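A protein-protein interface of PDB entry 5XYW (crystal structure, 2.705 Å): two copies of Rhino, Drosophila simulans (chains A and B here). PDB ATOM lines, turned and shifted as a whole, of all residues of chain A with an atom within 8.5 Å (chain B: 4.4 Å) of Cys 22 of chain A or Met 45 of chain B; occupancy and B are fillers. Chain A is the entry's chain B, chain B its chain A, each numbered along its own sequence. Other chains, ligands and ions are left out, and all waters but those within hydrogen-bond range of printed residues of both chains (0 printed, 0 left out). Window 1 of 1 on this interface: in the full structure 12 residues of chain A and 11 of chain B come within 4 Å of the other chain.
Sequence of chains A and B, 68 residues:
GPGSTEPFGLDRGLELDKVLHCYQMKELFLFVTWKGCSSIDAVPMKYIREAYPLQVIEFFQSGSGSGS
Of chain B, only Met 45 (3.9 Å) comes within 4 Å of Cys 22 of chain A. Of the printed residues of chain B, Gln 24 of chain A touches Leu 28 (3.9 Å). Printed residues of chain B within 4 Å of Leu 28 of chain A: Leu 28. Leu 30 of chain A touches none of the printed residues of chain B. Val 43 of chain B touches none of the printed residues of chain A. Met 45 of chain B touches just one residue of chain A: Cys 22 (3.9 Å). Of the printed residues of chain A, Arg 49 of chain B touches Phe 59 (3.1 Å) and Phe 60 (2.8 Å). Printed residues of chain A within 4 Å of Val 56 of chain B: Phe 60 (3.8 Å). Of the printed residues of chain A, Phe 60 of chain B touches Met 45. The nearest printed residue of chain A that does not touch Phe 60 of chain B is Leu 28 of chain A (4.02 Å).
The guanidinium group (NH2) of Arg 49 of chain B lies within hydrogen-bond range of the backbone carbonyl oxygen (O) of Phe 59 of chain A, 3.1 Å away. The backbone carbonyl oxygen (O) of Phe 60 of chain A lies close to the guanidinium group (NE) of Arg 49 of chain B, at 3.2 Å.
Of the 19 printed residues of chain A, 6 touch a printed residue of chain B. Hydrophobic or aromatic side chains of chain A that line the printed part of chain B: Leu 28, Met 45, Phe 59 and Phe 60. Of the 10 printed residues of chain B, 5 touch a printed residue of chain A. Printed residues of chain B that touch a printed residue of chain A: Leu 28, Met 45, Arg 49, Val 56 and Phe 60. Hydrophobic or aromatic side chains of chain B that line the printed part of chain A: Leu 28, Met 45, Val 56 and Phe 60.
Among the printed residues, merely in contact across the chains: Met 45 of chain A with Phe 60 of chain B, Phe 60 of chain A with Val 56 of chain B, Gln 24 of chain A with Leu 28 of chain B, Cys 22 of chain A with Met 45 of chain B and Leu 28 of chain A with Leu 28 of chain B.
The backbone carbonyl oxygen (O) of Leu 28 of chain B lies within hydrogen-bond range of the backbone NH (N) of Met 45 of chain B (2.8 Å). O of Glu 27 of chain A lies close to OE1 of Gln 24 of chain A (3.0 Å). The backbone NH (N) of Leu 28 of chain A sits at hydrogen-bond distance from the side-chain amide oxygen (OE1) of Gln 24 of chain A, at 3.2 Å. O of Leu 28 of chain A is in hydrogen-bond range of N of Met 45 of chain A, at 3.0 Å.
Leu 28 of chain A touches its own counterpart, Leu 28 of chain B. Met 45 of chain A touches Phe 60 of chain B, but with the chains exchanged Phe 60 of chain A does not touch Met 45 of chain B (4.4 Å). 4 positions are printed for both chains. Of the 7 pairs that touch across the chains among the printed residues, 1 has its exchanged pair printed and touching as well.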
ATOM      1  N   VAL A  19     -12.850 -16.837  37.851  1.00  0.00           N
ATOM      2  CA  VAL A  19     -11.989 -16.488  36.747  1.00  0.00           C
ATOM      3  C   VAL A  19     -12.868 -15.922  35.634  1.00  0.00           C
ATOM      4  O   VAL A  19     -13.643 -16.647  34.999  1.00  0.00           O
ATOM      5  CB  VAL A  19     -11.199 -17.676  36.251  1.00  0.00           C
ATOM      6  CG1 VAL A  19     -10.387 -17.274  35.025  1.00  0.00           C
ATOM      7  CG2 VAL A  19     -10.305 -18.183  37.352  1.00  0.00           C
ATOM      8  N   LEU A  20     -12.733 -14.616  35.408  1.00  0.00           N
ATOM      9  CA  LEU A  20     -13.699 -13.850  34.622  1.00  0.00           C
ATOM     10  C   LEU A  20     -13.501 -13.897  33.118  1.00  0.00           C
ATOM     11  O   LEU A  20     -14.466 -13.942  32.360  1.00  0.00           O
ATOM     12  CB  LEU A  20     -13.667 -12.399  35.059  1.00  0.00           C
ATOM     13  CG  LEU A  20     -13.954 -12.216  36.530  1.00  0.00           C
ATOM     14  CD1 LEU A  20     -13.972 -10.741  36.837  1.00  0.00           C
ATOM     15  CD2 LEU A  20     -15.285 -12.873  36.858  1.00  0.00           C
ATOM     16  N   HIS A  21     -12.250 -13.882  32.693  1.00  0.00           N
ATOM     17  CA  HIS A  21     -11.933 -13.640  31.298  1.00  0.00           C
ATOM     18  C   HIS A  21     -10.439 -13.860  31.133  1.00  0.00           C
ATOM     19  O   HIS A  21      -9.722 -14.122  32.119  1.00  0.00           O
ATOM     20  CB  HIS A  21     -12.357 -12.213  30.903  1.00  0.00           C
ATOM     21  CG  HIS A  21     -12.027 -11.832  29.497  1.00  0.00           C
ATOM     22  ND1 HIS A  21     -12.426 -12.585  28.406  1.00  0.00           N
ATOM     23  CD2 HIS A  21     -11.327 -10.789  28.995  1.00  0.00           C
ATOM     24  CE1 HIS A  21     -11.984 -12.019  27.297  1.00  0.00           C
ATOM     25  NE2 HIS A  21     -11.318 -10.924  27.632  1.00  0.00           N
ATOM     26  N   CYS A  22      -9.957 -13.781  29.902  1.00  0.00           N
ATOM     27  CA  CYS A  22      -8.530 -13.899  29.688  1.00  0.00           C
ATOM     28  C   CYS A  22      -8.070 -13.185  28.420  1.00  0.00           C
ATOM     29  O   CYS A  22      -8.825 -13.023  27.463  1.00  0.00           O
ATOM     30  CB  CYS A  22      -8.114 -15.376  29.633  1.00  0.00           C
ATOM     31  SG  CYS A  22      -8.428 -16.195  28.026  1.00  0.00           S
ATOM     32  N   TYR A  23      -6.805 -12.787  28.405  1.00  0.00           N
ATOM     33  CA  TYR A  23      -6.245 -12.139  27.230  1.00  0.00           C
ATOM     34  C   TYR A  23      -4.807 -12.597  27.020  1.00  0.00           C
ATOM     35  O   TYR A  23      -4.051 -12.715  27.986  1.00  0.00           O
ATOM     36  CB  TYR A  23      -6.330 -10.617  27.417  1.00  0.00           C
ATOM     37  CG  TYR A  23      -6.038  -9.744  26.209  1.00  0.00           C
ATOM     38  CD1 TYR A  23      -4.763  -9.230  25.995  1.00  0.00           C
ATOM     39  CD2 TYR A  23      -7.044  -9.395  25.310  1.00  0.00           C
ATOM     40  CE1 TYR A  23      -4.491  -8.416  24.922  1.00  0.00           C
ATOM     41  CE2 TYR A  23      -6.777  -8.570  24.214  1.00  0.00           C
ATOM     42  CZ  TYR A  23      -5.495  -8.088  24.030  1.00  0.00           C
ATOM     43  OH  TYR A  23      -5.199  -7.270  22.956  1.00  0.00           O
ATOM     44  N   GLN A  24      -4.425 -12.868  25.776  1.00  0.00           N
ATOM     45  CA  GLN A  24      -3.014 -13.120  25.461  1.00  0.00           C
ATOM     46  C   GLN A  24      -2.282 -11.863  24.978  1.00  0.00           C
ATOM     47  O   GLN A  24      -2.721 -11.230  24.029  1.00  0.00           O
ATOM     48  CB  GLN A  24      -2.882 -14.216  24.390  1.00  0.00           C
ATOM     49  CG  GLN A  24      -1.578 -14.161  23.552  1.00  0.00           C
ATOM     50  CD  GLN A  24      -0.353 -14.726  24.275  1.00  0.00           C
ATOM     51  OE1 GLN A  24      -0.470 -15.324  25.339  1.00  0.00           O
ATOM     52  NE2 GLN A  24       0.825 -14.543  23.688  1.00  0.00           N
ATOM     53  N   MET A  25      -1.177 -11.502  25.622  1.00  0.00           N
ATOM     54  CA  MET A  25      -0.229 -10.596  24.976  1.00  0.00           C
ATOM     55  C   MET A  25       1.144 -11.261  24.818  1.00  0.00           C
ATOM     56  O   MET A  25       1.530 -11.666  23.708  1.00  0.00           O
ATOM     57  CB  MET A  25      -0.087  -9.274  25.732  1.00  0.00           C
ATOM     58  CG  MET A  25       0.744  -8.230  24.941  1.00  0.00           C
ATOM     59  SD  MET A  25       0.109  -6.570  25.082  1.00  0.00           S
ATOM     60  CE  MET A  25      -1.547  -6.826  24.479  1.00  0.00           C
ATOM     61  N   GLU A  27       2.265 -13.537  27.609  1.00  0.00           N
ATOM     62  CA  GLU A  27       1.695 -14.716  28.234  1.00  0.00           C
ATOM     63  C   GLU A  27       0.182 -14.648  28.170  1.00  0.00           C
ATOM     64  O   GLU A  27      -0.393 -13.606  27.804  1.00  0.00           O
ATOM     65  CB  GLU A  27       2.153 -14.827  29.678  1.00  0.00           C
ATOM     66  CG  GLU A  27       3.640 -15.012  29.807  1.00  0.00           C
ATOM     67  CD  GLU A  27       4.043 -15.384  31.214  1.00  0.00           C
ATOM     68  OE1 GLU A  27       3.347 -14.939  32.150  1.00  0.00           O
ATOM     69  OE2 GLU A  27       5.043 -16.125  31.382  1.00  0.00           O
ATOM     70  N   LEU A  28      -0.470 -15.757  28.506  1.00  0.00           N
ATOM     71  CA  LEU A  28      -1.908 -15.690  28.676  1.00  0.00           C
ATOM     72  C   LEU A  28      -2.149 -15.137  30.072  1.00  0.00           C
ATOM     73  O   LEU A  28      -1.393 -15.406  30.997  1.00  0.00           O
ATOM     74  CB  LEU A  28      -2.590 -17.034  28.479  1.00  0.00           C
ATOM     75  CG  LEU A  28      -4.112 -16.968  28.622  1.00  0.00           C
ATOM     76  CD1 LEU A  28      -4.782 -16.335  27.366  1.00  0.00           C
ATOM     77  CD2 LEU A  28      -4.716 -18.350  28.958  1.00  0.00           C
ATOM     78  N   PHE A  29      -3.170 -14.302  30.190  1.00  0.00           N
ATOM     79  CA  PHE A  29      -3.524 -13.703  31.460  1.00  0.00           C
ATOM     80  C   PHE A  29      -4.950 -14.043  31.788  1.00  0.00           C
ATOM     81  O   PHE A  29      -5.825 -14.020  30.918  1.00  0.00           O
ATOM     82  CB  PHE A  29      -3.371 -12.182  31.433  1.00  0.00           C
ATOM     83  CG  PHE A  29      -1.959 -11.711  31.325  1.00  0.00           C
ATOM     84  CD1 PHE A  29      -1.386 -11.482  30.083  1.00  0.00           C
ATOM     85  CD2 PHE A  29      -1.210 -11.473  32.465  1.00  0.00           C
ATOM     86  CE1 PHE A  29      -0.082 -11.025  29.979  1.00  0.00           C
ATOM     87  CE2 PHE A  29       0.087 -11.023  32.372  1.00  0.00           C
ATOM     88  CZ  PHE A  29       0.652 -10.798  31.123  1.00  0.00           C
ATOM     89  N   LEU A  30      -5.173 -14.351  33.049  1.00  0.00           N
ATOM     90  CA  LEU A  30      -6.517 -14.475  33.574  1.00  0.00           C
ATOM     91  C   LEU A  30      -6.876 -13.200  34.321  1.00  0.00           C
ATOM     92  O   LEU A  30      -6.025 -12.571  34.972  1.00  0.00           O
ATOM     93  CB  LEU A  30      -6.638 -15.691  34.491  1.00  0.00           C
ATOM     94  CG  LEU A  30      -6.209 -16.990  33.799  1.00  0.00           C
ATOM     95  CD1 LEU A  30      -6.110 -18.147  34.806  1.00  0.00           C
ATOM     96  CD2 LEU A  30      -7.135 -17.330  32.606  1.00  0.00           C
ATOM     97  N   PHE A  31      -8.138 -12.815  34.216  1.00  0.00           N
ATOM     98  CA  PHE A  31      -8.624 -11.729  35.031  1.00  0.00           C
ATOM     99  C   PHE A  31      -9.499 -12.299  36.147  1.00  0.00           C
ATOM    100  O   PHE A  31     -10.620 -12.775  35.923  1.00  0.00           O
ATOM    101  CB  PHE A  31      -9.349 -10.715  34.160  1.00  0.00           C
ATOM    102  CG  PHE A  31      -8.585 -10.368  32.930  1.00  0.00           C
ATOM    103  CD1 PHE A  31      -7.481  -9.540  33.008  1.00  0.00           C
ATOM    104  CD2 PHE A  31      -8.937 -10.911  31.697  1.00  0.00           C
ATOM    105  CE1 PHE A  31      -6.760  -9.234  31.879  1.00  0.00           C
ATOM    106  CE2 PHE A  31      -8.210 -10.612  30.568  1.00  0.00           C
ATOM    107  CZ  PHE A  31      -7.120  -9.766  30.660  1.00  0.00           C
ATOM    108  N   VAL A  32      -8.951 -12.264  37.353  1.00  0.00           N
ATOM    109  CA  VAL A  32      -9.538 -12.963  38.476  1.00  0.00           C
ATOM    110  C   VAL A  32      -9.983 -12.020  39.566  1.00  0.00           C
ATOM    111  O   VAL A  32      -9.564 -10.866  39.622  1.00  0.00           O
ATOM    112  CB  VAL A  32      -8.549 -13.957  39.091  1.00  0.00           C
ATOM    113  CG1 VAL A  32      -8.403 -15.190  38.200  1.00  0.00           C
ATOM    114  CG2 VAL A  32      -7.211 -13.265  39.338  1.00  0.00           C
ATOM    115  N   ASP A  41      -8.110  -8.456  38.926  1.00  0.00           N
ATOM    116  CA  ASP A  41      -6.685  -8.425  38.679  1.00  0.00           C
ATOM    117  C   ASP A  41      -6.317  -9.222  37.438  1.00  0.00           C
ATOM    118  O   ASP A  41      -7.059 -10.102  37.011  1.00  0.00           O
ATOM    119  CB  ASP A  41      -5.930  -8.942  39.890  1.00  0.00           C
ATOM    120  CG  ASP A  41      -4.488  -8.477  39.910  1.00  0.00           C
ATOM    121  OD1 ASP A  41      -4.207  -7.311  39.522  1.00  0.00           O
ATOM    122  OD2 ASP A  41      -3.629  -9.289  40.312  1.00  0.00           O
ATOM    123  N   ALA A  42      -5.175  -8.881  36.849  1.00  0.00           N
ATOM    124  CA  ALA A  42      -4.671  -9.578  35.673  1.00  0.00           C
ATOM    125  C   ALA A  42      -3.381 -10.309  36.030  1.00  0.00           C
ATOM    126  O   ALA A  42      -2.414  -9.697  36.488  1.00  0.00           O
ATOM    127  CB  ALA A  42      -4.445  -8.601  34.500  1.00  0.00           C
ATOM    128  N   VAL A  43      -3.377 -11.626  35.827  1.00  0.00           N
ATOM    129  CA  VAL A  43      -2.270 -12.475  36.269  1.00  0.00           C
ATOM    130  C   VAL A  43      -1.963 -13.561  35.242  1.00  0.00           C
ATOM    131  O   VAL A  43      -2.877 -14.117  34.657  1.00  0.00           O
ATOM    132  CB  VAL A  43      -2.608 -13.140  37.621  1.00  0.00           C
ATOM    133  CG1 VAL A  43      -1.461 -14.040  38.105  1.00  0.00           C
ATOM    134  CG2 VAL A  43      -2.994 -12.083  38.661  1.00  0.00           C
ATOM    135  N   MET A  45      -1.703 -16.944  33.588  1.00  0.00           N
ATOM    136  CA  MET A  45      -2.493 -18.133  33.848  1.00  0.00           C
ATOM    137  C   MET A  45      -1.653 -19.208  34.535  1.00  0.00           C
ATOM    138  O   MET A  45      -2.180 -20.010  35.282  1.00  0.00           O
ATOM    139  CB  MET A  45      -3.093 -18.664  32.541  1.00  0.00           C
ATOM    140  CG  MET A  45      -3.732 -20.074  32.615  1.00  0.00           C
ATOM    141  SD  MET A  45      -2.508 -21.386  32.493  1.00  0.00           S
ATOM    142  CE  MET A  45      -2.454 -21.695  30.736  1.00  0.00           C
ATOM    143  N   PHE A  59     -12.540 -23.057  34.088  1.00  0.00           N
ATOM    144  CA  PHE A  59     -12.718 -21.872  33.281  1.00  0.00           C
ATOM    145  C   PHE A  59     -12.511 -22.209  31.810  1.00  0.00           C
ATOM    146  O   PHE A  59     -13.347 -21.887  30.964  1.00  0.00           O
ATOM    147  CB  PHE A  59     -11.756 -20.768  33.717  1.00  0.00           C
ATOM    148  CG  PHE A  59     -11.622 -19.667  32.721  1.00  0.00           C
ATOM    149  CD1 PHE A  59     -12.541 -18.629  32.689  1.00  0.00           C
ATOM    150  CD2 PHE A  59     -10.575 -19.667  31.812  1.00  0.00           C
ATOM    151  CE1 PHE A  59     -12.412 -17.607  31.765  1.00  0.00           C
ATOM    152  CE2 PHE A  59     -10.445 -18.665  30.884  1.00  0.00           C
ATOM    153  CZ  PHE A  59     -11.358 -17.631  30.858  1.00  0.00           C
ATOM    154  N   PHE A  60     -11.399 -22.868  31.509  1.00  0.00           N
ATOM    155  CA  PHE A  60     -11.111 -23.218  30.129  1.00  0.00           C
ATOM    156  C   PHE A  60     -12.206 -24.079  29.490  1.00  0.00           C
ATOM    157  O   PHE A  60     -12.405 -24.013  28.282  1.00  0.00           O
ATOM    158  CB  PHE A  60      -9.769 -23.930  30.041  1.00  0.00           C
ATOM    159  CG  PHE A  60      -8.587 -23.006  30.093  1.00  0.00           C
ATOM    160  CD1 PHE A  60      -7.795 -22.806  28.970  1.00  0.00           C
ATOM    161  CD2 PHE A  60      -8.265 -22.331  31.256  1.00  0.00           C
ATOM    162  CE1 PHE A  60      -6.695 -21.961  29.016  1.00  0.00           C
ATOM    163  CE2 PHE A  60      -7.171 -21.479  31.304  1.00  0.00           C
ATOM    164  CZ  PHE A  60      -6.384 -21.301  30.190  1.00  0.00           C
ATOM    165  N   LEU B  28      -9.337 -14.218  20.565  1.00  0.00           N
ATOM    166  CA  LEU B  28      -8.080 -14.923  20.517  1.00  0.00           C
ATOM    167  C   LEU B  28      -8.192 -16.036  19.476  1.00  0.00           C
ATOM    168  O   LEU B  28      -9.185 -16.763  19.422  1.00  0.00           O
ATOM    169  CB  LEU B  28      -7.745 -15.467  21.897  1.00  0.00           C
ATOM    170  CG  LEU B  28      -6.406 -16.133  22.163  1.00  0.00           C
ATOM    171  CD1 LEU B  28      -5.236 -15.367  21.569  1.00  0.00           C
ATOM    172  CD2 LEU B  28      -6.244 -16.253  23.648  1.00  0.00           C
ATOM    173  N   VAL B  43      -8.778 -20.867  14.515  1.00  0.00           N
ATOM    174  CA  VAL B  43      -9.970 -21.285  15.218  1.00  0.00           C
ATOM    175  C   VAL B  43     -10.069 -20.420  16.438  1.00  0.00           C
ATOM    176  O   VAL B  43      -9.078 -20.237  17.126  1.00  0.00           O
ATOM    177  CB  VAL B  43      -9.917 -22.762  15.597  1.00  0.00           C
ATOM    178  CG1 VAL B  43     -11.170 -23.152  16.382  1.00  0.00           C
ATOM    179  CG2 VAL B  43      -9.754 -23.621  14.350  1.00  0.00           C
ATOM    180  N   PRO B  44     -11.250 -19.847  16.694  1.00  0.00           N
ATOM    181  CA  PRO B  44     -11.382 -19.027  17.898  1.00  0.00           C
ATOM    182  C   PRO B  44     -11.108 -19.822  19.172  1.00  0.00           C
ATOM    183  O   PRO B  44     -11.515 -20.980  19.298  1.00  0.00           O
ATOM    184  CB  PRO B  44     -12.838 -18.549  17.838  1.00  0.00           C
ATOM    185  CG  PRO B  44     -13.183 -18.598  16.414  1.00  0.00           C
ATOM    186  CD  PRO B  44     -12.450 -19.765  15.845  1.00  0.00           C
ATOM    187  N   MET B  45     -10.389 -19.185  20.087  1.00  0.00           N
ATOM    188  CA  MET B  45     -10.000 -19.762  21.364  1.00  0.00           C
ATOM    189  C   MET B  45     -11.131 -20.464  22.103  1.00  0.00           C
ATOM    190  O   MET B  45     -10.958 -21.555  22.614  1.00  0.00           O
ATOM    191  CB  MET B  45      -9.426 -18.666  22.255  1.00  0.00           C
ATOM    192  CG  MET B  45      -9.602 -18.922  23.736  1.00  0.00           C
ATOM    193  SD  MET B  45      -8.545 -20.219  24.393  1.00  0.00           S
ATOM    194  CE  MET B  45      -7.863 -19.278  25.760  1.00  0.00           C
ATOM    195  N   LYS B  46     -12.284 -19.815  22.165  1.00  0.00           N
ATOM    196  CA  LYS B  46     -13.424 -20.318  22.915  1.00  0.00           C
ATOM    197  C   LYS B  46     -13.870 -21.694  22.429  1.00  0.00           C
ATOM    198  O   LYS B  46     -14.068 -22.629  23.221  1.00  0.00           O
ATOM    199  CB  LYS B  46     -14.560 -19.306  22.819  1.00  0.00           C
ATOM    200  CG  LYS B  46     -14.057 -17.857  22.927  1.00  0.00           C
ATOM    201  CD  LYS B  46     -15.178 -16.822  22.857  1.00  0.00           C
ATOM    202  CE  LYS B  46     -14.657 -15.423  23.205  1.00  0.00           C
ATOM    203  NZ  LYS B  46     -15.653 -14.333  22.947  1.00  0.00           N
ATOM    204  N   TYR B  47     -14.005 -21.826  21.119  1.00  0.00           N
ATOM    205  CA  TYR B  47     -14.415 -23.090  20.518  1.00  0.00           C
ATOM    206  C   TYR B  47     -13.446 -24.207  20.891  1.00  0.00           C
ATOM    207  O   TYR B  47     -13.828 -25.232  21.460  1.00  0.00           O
ATOM    208  CB  TYR B  47     -14.487 -22.974  18.989  1.00  0.00           C
ATOM    209  CG  TYR B  47     -15.528 -22.026  18.427  1.00  0.00           C
ATOM    210  CD1 TYR B  47     -16.073 -21.005  19.195  1.00  0.00           C
ATOM    211  CD2 TYR B  47     -15.966 -22.158  17.114  1.00  0.00           C
ATOM    212  CE1 TYR B  47     -17.020 -20.135  18.673  1.00  0.00           C
ATOM    213  CE2 TYR B  47     -16.916 -21.293  16.583  1.00  0.00           C
ATOM    214  CZ  TYR B  47     -17.438 -20.280  17.370  1.00  0.00           C
ATOM    215  OH  TYR B  47     -18.382 -19.408  16.858  1.00  0.00           O
ATOM    216  N   ILE B  48     -12.182 -23.986  20.561  1.00  0.00           N
ATOM    217  CA  ILE B  48     -11.155 -24.992  20.746  1.00  0.00           C
ATOM    218  C   ILE B  48     -11.035 -25.353  22.231  1.00  0.00           C
ATOM    219  O   ILE B  48     -10.815 -26.501  22.587  1.00  0.00           O
ATOM    220  CB  ILE B  48      -9.803 -24.488  20.172  1.00  0.00           C
ATOM    221  CG1 ILE B  48      -8.823 -25.631  19.944  1.00  0.00           C
ATOM    222  CG2 ILE B  48      -9.201 -23.401  21.031  1.00  0.00           C
ATOM    223  CD1 ILE B  48      -8.992 -26.280  18.599  1.00  0.00           C
ATOM    224  N   ARG B  49     -11.246 -24.365  23.089  1.00  0.00           N
ATOM    225  CA  ARG B  49     -11.008 -24.507  24.513  1.00  0.00           C
ATOM    226  C   ARG B  49     -12.145 -25.240  25.171  1.00  0.00           C
ATOM    227  O   ARG B  49     -11.964 -25.832  26.217  1.00  0.00           O
ATOM    228  CB  ARG B  49     -10.832 -23.142  25.182  1.00  0.00           C
ATOM    229  CG  ARG B  49     -12.149 -22.486  25.511  1.00  0.00           C
ATOM    230  CD  ARG B  49     -12.009 -21.161  26.205  1.00  0.00           C
ATOM    231  NE  ARG B  49     -13.055 -21.034  27.211  1.00  0.00           N
ATOM    232  CZ  ARG B  49     -13.346 -19.908  27.841  1.00  0.00           C
ATOM    233  NH1 ARG B  49     -12.669 -18.812  27.555  1.00  0.00           N
ATOM    234  NH2 ARG B  49     -14.312 -19.879  28.750  1.00  0.00           N
ATOM    235  N   VAL B  56      -4.981 -27.092  25.006  1.00  0.00           N
ATOM    236  CA  VAL B  56      -4.888 -25.636  25.043  1.00  0.00           C
ATOM    237  C   VAL B  56      -3.985 -25.134  26.157  1.00  0.00           C
ATOM    238  O   VAL B  56      -3.007 -24.409  25.901  1.00  0.00           O
ATOM    239  CB  VAL B  56      -6.259 -24.974  25.248  1.00  0.00           C
ATOM    240  CG1 VAL B  56      -6.086 -23.517  25.630  1.00  0.00           C
ATOM    241  CG2 VAL B  56      -7.129 -25.104  23.997  1.00  0.00           C
ATOM    242  N   PHE B  60      -0.467 -22.919  26.251  1.00  0.00           N
ATOM    243  CA  PHE B  60      -0.152 -21.652  26.899  1.00  0.00           C
ATOM    244  C   PHE B  60       0.822 -21.763  28.082  1.00  0.00           C
ATOM    245  O   PHE B  60       1.519 -20.801  28.418  1.00  0.00           O
ATOM    246  CB  PHE B  60      -1.437 -20.975  27.356  1.00  0.00           C
ATOM    247  CG  PHE B  60      -2.273 -20.476  26.228  1.00  0.00           C
ATOM    248  CD1 PHE B  60      -1.790 -19.471  25.386  1.00  0.00           C
ATOM    249  CD2 PHE B  60      -3.536 -21.005  25.991  1.00  0.00           C
ATOM    250  CE1 PHE B  60      -2.549 -19.004  24.339  1.00  0.00           C
ATOM    251  CE2 PHE B  60      -4.310 -20.536  24.933  1.00  0.00           C
ATOM    252  CZ  PHE B  60      -3.812 -19.543  24.111  1.00  0.00           C
